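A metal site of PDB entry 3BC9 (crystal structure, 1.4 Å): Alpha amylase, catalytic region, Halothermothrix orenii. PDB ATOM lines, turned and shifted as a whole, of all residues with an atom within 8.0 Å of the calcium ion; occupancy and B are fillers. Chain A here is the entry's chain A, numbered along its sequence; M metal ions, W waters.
Water W1 lies within hydrogen-bond range of the backbone carbonyl oxygen of Asn 232 (2.8 Å) and the backbone carbonyl oxygen of Val 320 (3.2 Å).
OD1 of Asn 232 binds the calcium ion (2.3 Å). OD1 of Asp 313 is bound to the calcium ion. The backbone carbonyl oxygen (O) of His 354 binds the calcium ion (2.3 Å). OD1 of Asp 319 is bound to the calcium ion, 2.4 Å away. O of Asp 313 is bound to the calcium ion (2.4 Å). Water W1 is bound to the calcium ion (2.4 Å). The calcium ion has six donor atoms within binding distance.
The backbone NH (N) of Val 320 is in hydrogen-bond range of the backbone carbonyl oxygen (O) of Asn 232 (3.0 Å). The side-chain amide nitrogen of Asn 232 lies within hydrogen-bond range of a ring nitrogen (ND1) of His 233. OD2 of Asp 313 sits at hydrogen-bond distance from N of Asp 305 (2.8 Å). A ring nitrogen (ND1) of His 354 is in hydrogen-bond range of the backbone carbonyl oxygen (O) of Glu 312, at 2.8 Å. The backbone carbonyl oxygen of Asp 319 sits at hydrogen-bond distance from the backbone NH of Asp 283, at 2.8 Å.
Of the 23 residues printed, 4 come within 4 Å of the calcium ion. The nearest printed residue that does not touch the calcium ion is Tyr 314 (4.4 Å).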
ATOM      1  N   LEU A 231       7.826 -20.457  32.741  1.00  0.00           N
ATOM      2  CA  LEU A 231       7.765 -19.797  31.457  1.00  0.00           C
ATOM      3  C   LEU A 231       8.019 -20.727  30.256  1.00  0.00           C
ATOM      4  O   LEU A 231       7.957 -20.309  29.117  1.00  0.00           O
ATOM      5  CB  LEU A 231       8.648 -18.563  31.445  1.00  0.00           C
ATOM      6  CG  LEU A 231       8.453 -17.497  32.577  1.00  0.00           C
ATOM      7  CD1 LEU A 231       9.383 -16.300  32.393  1.00  0.00           C
ATOM      8  CD2 LEU A 231       6.851 -17.233  32.591  1.00  0.00           C
ATOM      9  N   ASN A 232       8.506 -21.917  30.531  1.00  0.00           N
ATOM     10  CA  ASN A 232       9.013 -22.727  29.437  1.00  0.00           C
ATOM     11  C   ASN A 232       7.882 -23.273  28.460  1.00  0.00           C
ATOM     12  O   ASN A 232       8.089 -23.339  27.236  1.00  0.00           O
ATOM     13  CB  ASN A 232       9.726 -23.952  30.031  1.00  0.00           C
ATOM     14  CG  ASN A 232      10.132 -24.922  28.987  1.00  0.00           C
ATOM     15  OD1 ASN A 232      10.990 -24.611  28.162  1.00  0.00           O
ATOM     16  ND2 ASN A 232       9.538 -26.088  28.997  1.00  0.00           N
ATOM     17  N   HIS A 233       6.712 -23.647  28.984  1.00  0.00           N
ATOM     18  CA  HIS A 233       5.753 -24.433  28.269  1.00  0.00           C
ATOM     19  C   HIS A 233       4.386 -24.024  28.698  1.00  0.00           C
ATOM     20  O   HIS A 233       4.189 -23.438  29.719  1.00  0.00           O
ATOM     21  CB  HIS A 233       6.016 -25.892  28.470  1.00  0.00           C
ATOM     22  CG  HIS A 233       5.957 -26.285  29.873  1.00  0.00           C
ATOM     23  ND1 HIS A 233       7.095 -26.512  30.615  1.00  0.00           N
ATOM     24  CD2 HIS A 233       4.913 -26.419  30.716  1.00  0.00           C
ATOM     25  CE1 HIS A 233       6.747 -26.776  31.860  1.00  0.00           C
ATOM     26  NE2 HIS A 233       5.420 -26.717  31.937  1.00  0.00           N
ATOM     27  N   ASP A 283       7.245 -23.429  19.516  1.00  0.00           N
ATOM     28  CA  ASP A 283       8.174 -24.065  18.639  1.00  0.00           C
ATOM     29  C   ASP A 283       7.850 -25.498  18.321  1.00  0.00           C
ATOM     30  O   ASP A 283       8.225 -26.015  17.274  1.00  0.00           O
ATOM     31  CB  ASP A 283       9.599 -24.047  19.201  1.00  0.00           C
ATOM     32  CG  ASP A 283      10.249 -22.666  19.097  1.00  0.00           C
ATOM     33  OD1 ASP A 283       9.939 -22.038  18.005  1.00  0.00           O
ATOM     34  OD2 ASP A 283      11.020 -22.135  19.997  1.00  0.00           O
ATOM     35  N   TRP A 304      14.303 -24.134  17.412  1.00  0.00           N
ATOM     36  CA  TRP A 304      14.478 -24.124  18.853  1.00  0.00           C
ATOM     37  C   TRP A 304      15.277 -22.872  19.213  1.00  0.00           C
ATOM     38  O   TRP A 304      16.217 -22.440  18.525  1.00  0.00           O
ATOM     39  CB  TRP A 304      15.183 -25.374  19.295  1.00  0.00           C
ATOM     40  CG  TRP A 304      14.493 -26.657  18.961  1.00  0.00           C
ATOM     41  CD1 TRP A 304      14.993 -27.666  18.244  1.00  0.00           C
ATOM     42  CD2 TRP A 304      13.177 -27.074  19.389  1.00  0.00           C
ATOM     43  NE1 TRP A 304      14.070 -28.671  18.145  1.00  0.00           N
ATOM     44  CE2 TRP A 304      12.957 -28.355  18.868  1.00  0.00           C
ATOM     45  CE3 TRP A 304      12.179 -26.486  20.149  1.00  0.00           C
ATOM     46  CZ2 TRP A 304      11.742 -29.019  19.031  1.00  0.00           C
ATOM     47  CZ3 TRP A 304      11.000 -27.131  20.316  1.00  0.00           C
ATOM     48  CH2 TRP A 304      10.786 -28.407  19.767  1.00  0.00           C
ATOM     49  N   ASP A 305      14.909 -22.304  20.349  1.00  0.00           N
ATOM     50  CA  ASP A 305      15.460 -21.076  20.836  1.00  0.00           C
ATOM     51  C   ASP A 305      16.897 -21.330  21.337  1.00  0.00           C
ATOM     52  O   ASP A 305      17.321 -22.444  21.581  1.00  0.00           O
ATOM     53  CB  ASP A 305      14.573 -20.487  21.897  1.00  0.00           C
ATOM     54  CG  ASP A 305      13.164 -20.130  21.425  1.00  0.00           C
ATOM     55  OD1 ASP A 305      13.086 -19.771  20.238  1.00  0.00           O
ATOM     56  OD2 ASP A 305      12.293 -20.134  22.347  1.00  0.00           O
ATOM     57  N   THR A 307      19.742 -21.810  23.754  1.00  0.00           N
ATOM     58  CA  THR A 307      19.941 -22.251  25.129  1.00  0.00           C
ATOM     59  C   THR A 307      21.406 -22.512  25.364  1.00  0.00           C
ATOM     60  O   THR A 307      22.165 -22.723  24.416  1.00  0.00           O
ATOM     61  CB  THR A 307      19.114 -23.536  25.416  1.00  0.00           C
ATOM     62  OG1 THR A 307      19.348 -24.606  24.452  1.00  0.00           O
ATOM     63  CG2 THR A 307      17.561 -23.270  25.397  1.00  0.00           C
ATOM     64  N   GLU A 312      18.563 -27.798  24.014  1.00  0.00           N
ATOM     65  CA  GLU A 312      17.874 -28.052  25.270  1.00  0.00           C
ATOM     66  C   GLU A 312      16.595 -27.187  25.415  1.00  0.00           C
ATOM     67  O   GLU A 312      15.981 -27.149  26.499  1.00  0.00           O
ATOM     68  CB  GLU A 312      18.842 -27.857  26.502  1.00  0.00           C
ATOM     69  CG  GLU A 312      19.761 -29.022  26.732  1.00  0.00           C
ATOM     70  CD  GLU A 312      20.286 -29.077  28.192  1.00  0.00           C
ATOM     71  OE1 GLU A 312      20.380 -28.029  28.936  1.00  0.00           O
ATOM     72  OE2 GLU A 312      20.750 -30.186  28.540  1.00  0.00           O
ATOM     73  N   ASP A 313      16.173 -26.504  24.367  1.00  0.00           N
ATOM     74  CA  ASP A 313      14.907 -25.747  24.491  1.00  0.00           C
ATOM     75  C   ASP A 313      13.716 -26.689  24.813  1.00  0.00           C
ATOM     76  O   ASP A 313      12.898 -26.373  25.642  1.00  0.00           O
ATOM     77  CB  ASP A 313      14.622 -25.057  23.173  1.00  0.00           C
ATOM     78  CG  ASP A 313      13.527 -24.012  23.209  1.00  0.00           C
ATOM     79  OD1 ASP A 313      13.132 -23.574  24.304  1.00  0.00           O
ATOM     80  OD2 ASP A 313      13.155 -23.533  22.102  1.00  0.00           O
ATOM     81  N   TYR A 314      13.569 -27.859  24.163  1.00  0.00           N
ATOM     82  CA  TYR A 314      12.412 -28.668  24.338  1.00  0.00           C
ATOM     83  C   TYR A 314      12.542 -29.472  25.599  1.00  0.00           C
ATOM     84  O   TYR A 314      13.566 -30.210  25.800  1.00  0.00           O
ATOM     85  CB  TYR A 314      12.091 -29.576  23.145  1.00  0.00           C
ATOM     86  CG  TYR A 314      10.753 -30.139  23.356  1.00  0.00           C
ATOM     87  CD1 TYR A 314       9.645 -29.378  23.112  1.00  0.00           C
ATOM     88  CD2 TYR A 314      10.565 -31.329  23.995  1.00  0.00           C
ATOM     89  CE1 TYR A 314       8.413 -29.764  23.534  1.00  0.00           C
ATOM     90  CE2 TYR A 314       9.289 -31.787  24.323  1.00  0.00           C
ATOM     91  CZ  TYR A 314       8.265 -30.949  24.160  1.00  0.00           C
ATOM     92  OH  TYR A 314       6.981 -31.368  24.617  1.00  0.00           O
ATOM     93  N   LEU A 315      11.537 -29.403  26.475  1.00  0.00           N
ATOM     94  CA  LEU A 315      11.452 -30.253  27.699  1.00  0.00           C
ATOM     95  C   LEU A 315      10.136 -31.053  27.733  1.00  0.00           C
ATOM     96  O   LEU A 315      10.163 -32.277  27.768  1.00  0.00           O
ATOM     97  CB  LEU A 315      11.606 -29.359  28.950  1.00  0.00           C
ATOM     98  CG  LEU A 315      11.614 -30.052  30.313  1.00  0.00           C
ATOM     99  CD1 LEU A 315      12.904 -30.940  30.473  1.00  0.00           C
ATOM    100  CD2 LEU A 315      11.470 -28.963  31.401  1.00  0.00           C
ATOM    101  N   MET A 316       9.017 -30.343  27.690  1.00  0.00           N
ATOM    102  CA  MET A 316       7.722 -30.919  27.799  1.00  0.00           C
ATOM    103  C   MET A 316       6.671 -29.952  27.292  1.00  0.00           C
ATOM    104  O   MET A 316       6.859 -28.803  27.107  1.00  0.00           O
ATOM    105  CB  MET A 316       7.424 -31.393  29.241  1.00  0.00           C
ATOM    106  CG  MET A 316       7.315 -30.278  30.239  1.00  0.00           C
ATOM    107  SD  MET A 316       6.922 -30.861  31.908  1.00  0.00           S
ATOM    108  CE  MET A 316       8.439 -31.811  32.288  1.00  0.00           C
ATOM    109  N   ALA A 318       3.730 -27.858  25.229  1.00  0.00           N
ATOM    110  CA  ALA A 318       3.819 -27.077  24.039  1.00  0.00           C
ATOM    111  C   ALA A 318       4.918 -26.074  24.408  1.00  0.00           C
ATOM    112  O   ALA A 318       4.764 -25.266  25.363  1.00  0.00           O
ATOM    113  CB  ALA A 318       2.545 -26.322  23.715  1.00  0.00           C
ATOM    114  N   ASP A 319       6.064 -26.048  23.679  1.00  0.00           N
ATOM    115  CA  ASP A 319       7.233 -25.243  24.032  1.00  0.00           C
ATOM    116  C   ASP A 319       7.053 -23.838  23.510  1.00  0.00           C
ATOM    117  O   ASP A 319       6.925 -23.673  22.304  1.00  0.00           O
ATOM    118  CB  ASP A 319       8.465 -25.896  23.442  1.00  0.00           C
ATOM    119  CG  ASP A 319       9.735 -25.164  23.870  1.00  0.00           C
ATOM    120  OD1 ASP A 319      10.086 -25.433  25.012  1.00  0.00           O
ATOM    121  OD2 ASP A 319      10.282 -24.431  23.046  1.00  0.00           O
ATOM    122  N   VAL A 320       7.182 -22.870  24.381  1.00  0.00           N
ATOM    123  CA  VAL A 320       6.975 -21.476  24.006  1.00  0.00           C
ATOM    124  C   VAL A 320       8.064 -21.055  23.056  1.00  0.00           C
ATOM    125  O   VAL A 320       9.233 -21.380  23.256  1.00  0.00           O
ATOM    126  CB  VAL A 320       6.868 -20.538  25.181  1.00  0.00           C
ATOM    127  CG1 VAL A 320       6.665 -19.123  24.780  1.00  0.00           C
ATOM    128  CG2 VAL A 320       5.680 -21.028  26.078  1.00  0.00           C
ATOM    129  N   ASP A 321       7.687 -20.318  21.981  1.00  0.00           N
ATOM    130  CA  ASP A 321       8.617 -19.734  21.038  1.00  0.00           C
ATOM    131  C   ASP A 321       8.971 -18.356  21.478  1.00  0.00           C
ATOM    132  O   ASP A 321       8.217 -17.414  21.167  1.00  0.00           O
ATOM    133  CB  ASP A 321       8.055 -19.698  19.619  1.00  0.00           C
ATOM    134  CG  ASP A 321       8.947 -19.136  18.642  1.00  0.00           C
ATOM    135  OD1 ASP A 321      10.148 -18.893  18.937  1.00  0.00           O
ATOM    136  OD2 ASP A 321       8.522 -18.880  17.476  1.00  0.00           O
ATOM    137  N   TYR A 322      10.095 -18.170  22.186  1.00  0.00           N
ATOM    138  CA  TYR A 322      10.474 -16.862  22.679  1.00  0.00           C
ATOM    139  C   TYR A 322      11.162 -16.029  21.629  1.00  0.00           C
ATOM    140  O   TYR A 322      11.606 -14.915  21.952  1.00  0.00           O
ATOM    141  CB  TYR A 322      11.259 -16.948  23.983  1.00  0.00           C
ATOM    142  CG  TYR A 322      10.300 -17.218  25.137  1.00  0.00           C
ATOM    143  CD1 TYR A 322      10.294 -18.381  25.840  1.00  0.00           C
ATOM    144  CD2 TYR A 322       9.362 -16.262  25.470  1.00  0.00           C
ATOM    145  CE1 TYR A 322       9.386 -18.612  26.864  1.00  0.00           C
ATOM    146  CE2 TYR A 322       8.472 -16.461  26.518  1.00  0.00           C
ATOM    147  CZ  TYR A 322       8.451 -17.671  27.181  1.00  0.00           C
ATOM    148  OH  TYR A 322       7.581 -17.864  28.197  1.00  0.00           O
ATOM    149  N   ALA A 351      13.036 -24.149  35.386  1.00  0.00           N
ATOM    150  CA  ALA A 351      13.440 -24.727  34.081  1.00  0.00           C
ATOM    151  C   ALA A 351      14.242 -23.711  33.243  1.00  0.00           C
ATOM    152  O   ALA A 351      14.121 -23.720  31.997  1.00  0.00           O
ATOM    153  CB  ALA A 351      12.296 -25.408  33.270  1.00  0.00           C
ATOM    154  N   VAL A 352      15.067 -22.860  33.890  1.00  0.00           N
ATOM    155  CA  VAL A 352      15.656 -21.704  33.278  1.00  0.00           C
ATOM    156  C   VAL A 352      16.573 -22.089  32.153  1.00  0.00           C
ATOM    157  O   VAL A 352      16.684 -21.306  31.172  1.00  0.00           O
ATOM    158  CB  VAL A 352      16.234 -20.738  34.271  1.00  0.00           C
ATOM    159  CG1 VAL A 352      17.535 -21.226  34.751  1.00  0.00           C
ATOM    160  CG2 VAL A 352      16.232 -19.364  33.687  1.00  0.00           C
ATOM    161  N   LYS A 353      17.193 -23.257  32.218  1.00  0.00           N
ATOM    162  CA  LYS A 353      18.104 -23.619  31.176  1.00  0.00           C
ATOM    163  C   LYS A 353      17.477 -24.021  29.887  1.00  0.00           C
ATOM    164  O   LYS A 353      18.111 -24.134  28.884  1.00  0.00           O
ATOM    165  CB  LYS A 353      19.129 -24.579  31.627  1.00  0.00           C
ATOM    166  CG  LYS A 353      18.668 -25.919  31.777  1.00  0.00           C
ATOM    167  CD  LYS A 353      19.896 -26.772  32.273  1.00  0.00           C
ATOM    168  CE  LYS A 353      19.440 -28.207  32.358  1.00  0.00           C
ATOM    169  NZ  LYS A 353      20.481 -29.291  32.699  1.00  0.00           N
ATOM    170  N   HIS A 354      16.158 -24.166  29.912  1.00  0.00           N
ATOM    171  CA  HIS A 354      15.351 -24.601  28.771  1.00  0.00           C
ATOM    172  C   HIS A 354      14.635 -23.434  28.123  1.00  0.00           C
ATOM    173  O   HIS A 354      13.730 -23.673  27.284  1.00  0.00           O
ATOM    174  CB  HIS A 354      14.316 -25.680  29.185  1.00  0.00           C
ATOM    175  CG  HIS A 354      14.922 -26.853  29.860  1.00  0.00           C
ATOM    176  ND1 HIS A 354      15.619 -27.815  29.191  1.00  0.00           N
ATOM    177  CD2 HIS A 354      14.997 -27.177  31.169  1.00  0.00           C
ATOM    178  CE1 HIS A 354      16.075 -28.707  30.083  1.00  0.00           C
ATOM    179  NE2 HIS A 354      15.732 -28.335  31.297  1.00  0.00           N
ATOM    180  N   ILE A 355      14.935 -22.243  28.538  1.00  0.00           N
ATOM    181  CA  ILE A 355      14.310 -20.994  28.017  1.00  0.00           C
ATOM    182  C   ILE A 355      15.379 -20.107  27.361  1.00  0.00           C
ATOM    183  O   ILE A 355      16.492 -19.968  27.855  1.00  0.00           O
ATOM    184  CB  ILE A 355      13.638 -20.242  29.155  1.00  0.00           C
ATOM    185  CG1 ILE A 355      12.565 -21.141  29.771  1.00  0.00           C
ATOM    186  CG2 ILE A 355      12.981 -18.946  28.576  1.00  0.00           C
ATOM    187  CD1 ILE A 355      12.073 -20.579  31.100  1.00  0.00           C
ATOM    188  N   ASP A 356      15.050 -19.595  26.166  1.00  0.00           N
ATOM    189  CA  ASP A 356      15.937 -18.727  25.426  1.00  0.00           C
ATOM    190  C   ASP A 356      16.661 -17.790  26.372  1.00  0.00           C
ATOM    191  O   ASP A 356      16.044 -16.974  27.027  1.00  0.00           O
ATOM    192  CB  ASP A 356      15.143 -17.869  24.444  1.00  0.00           C
ATOM    193  CG  ASP A 356      16.020 -17.292  23.401  1.00  0.00           C
ATOM    194  OD1 ASP A 356      16.785 -16.410  23.755  1.00  0.00           O
ATOM    195  OD2 ASP A 356      16.226 -17.772  22.259  1.00  0.00           O
HETATM  196 CA    CA M   1      11.852 -24.292  26.067  1.00  0.00          CA
HETATM  197  O   HOH W   1      10.441 -22.361  26.000  1.00  0.00           O
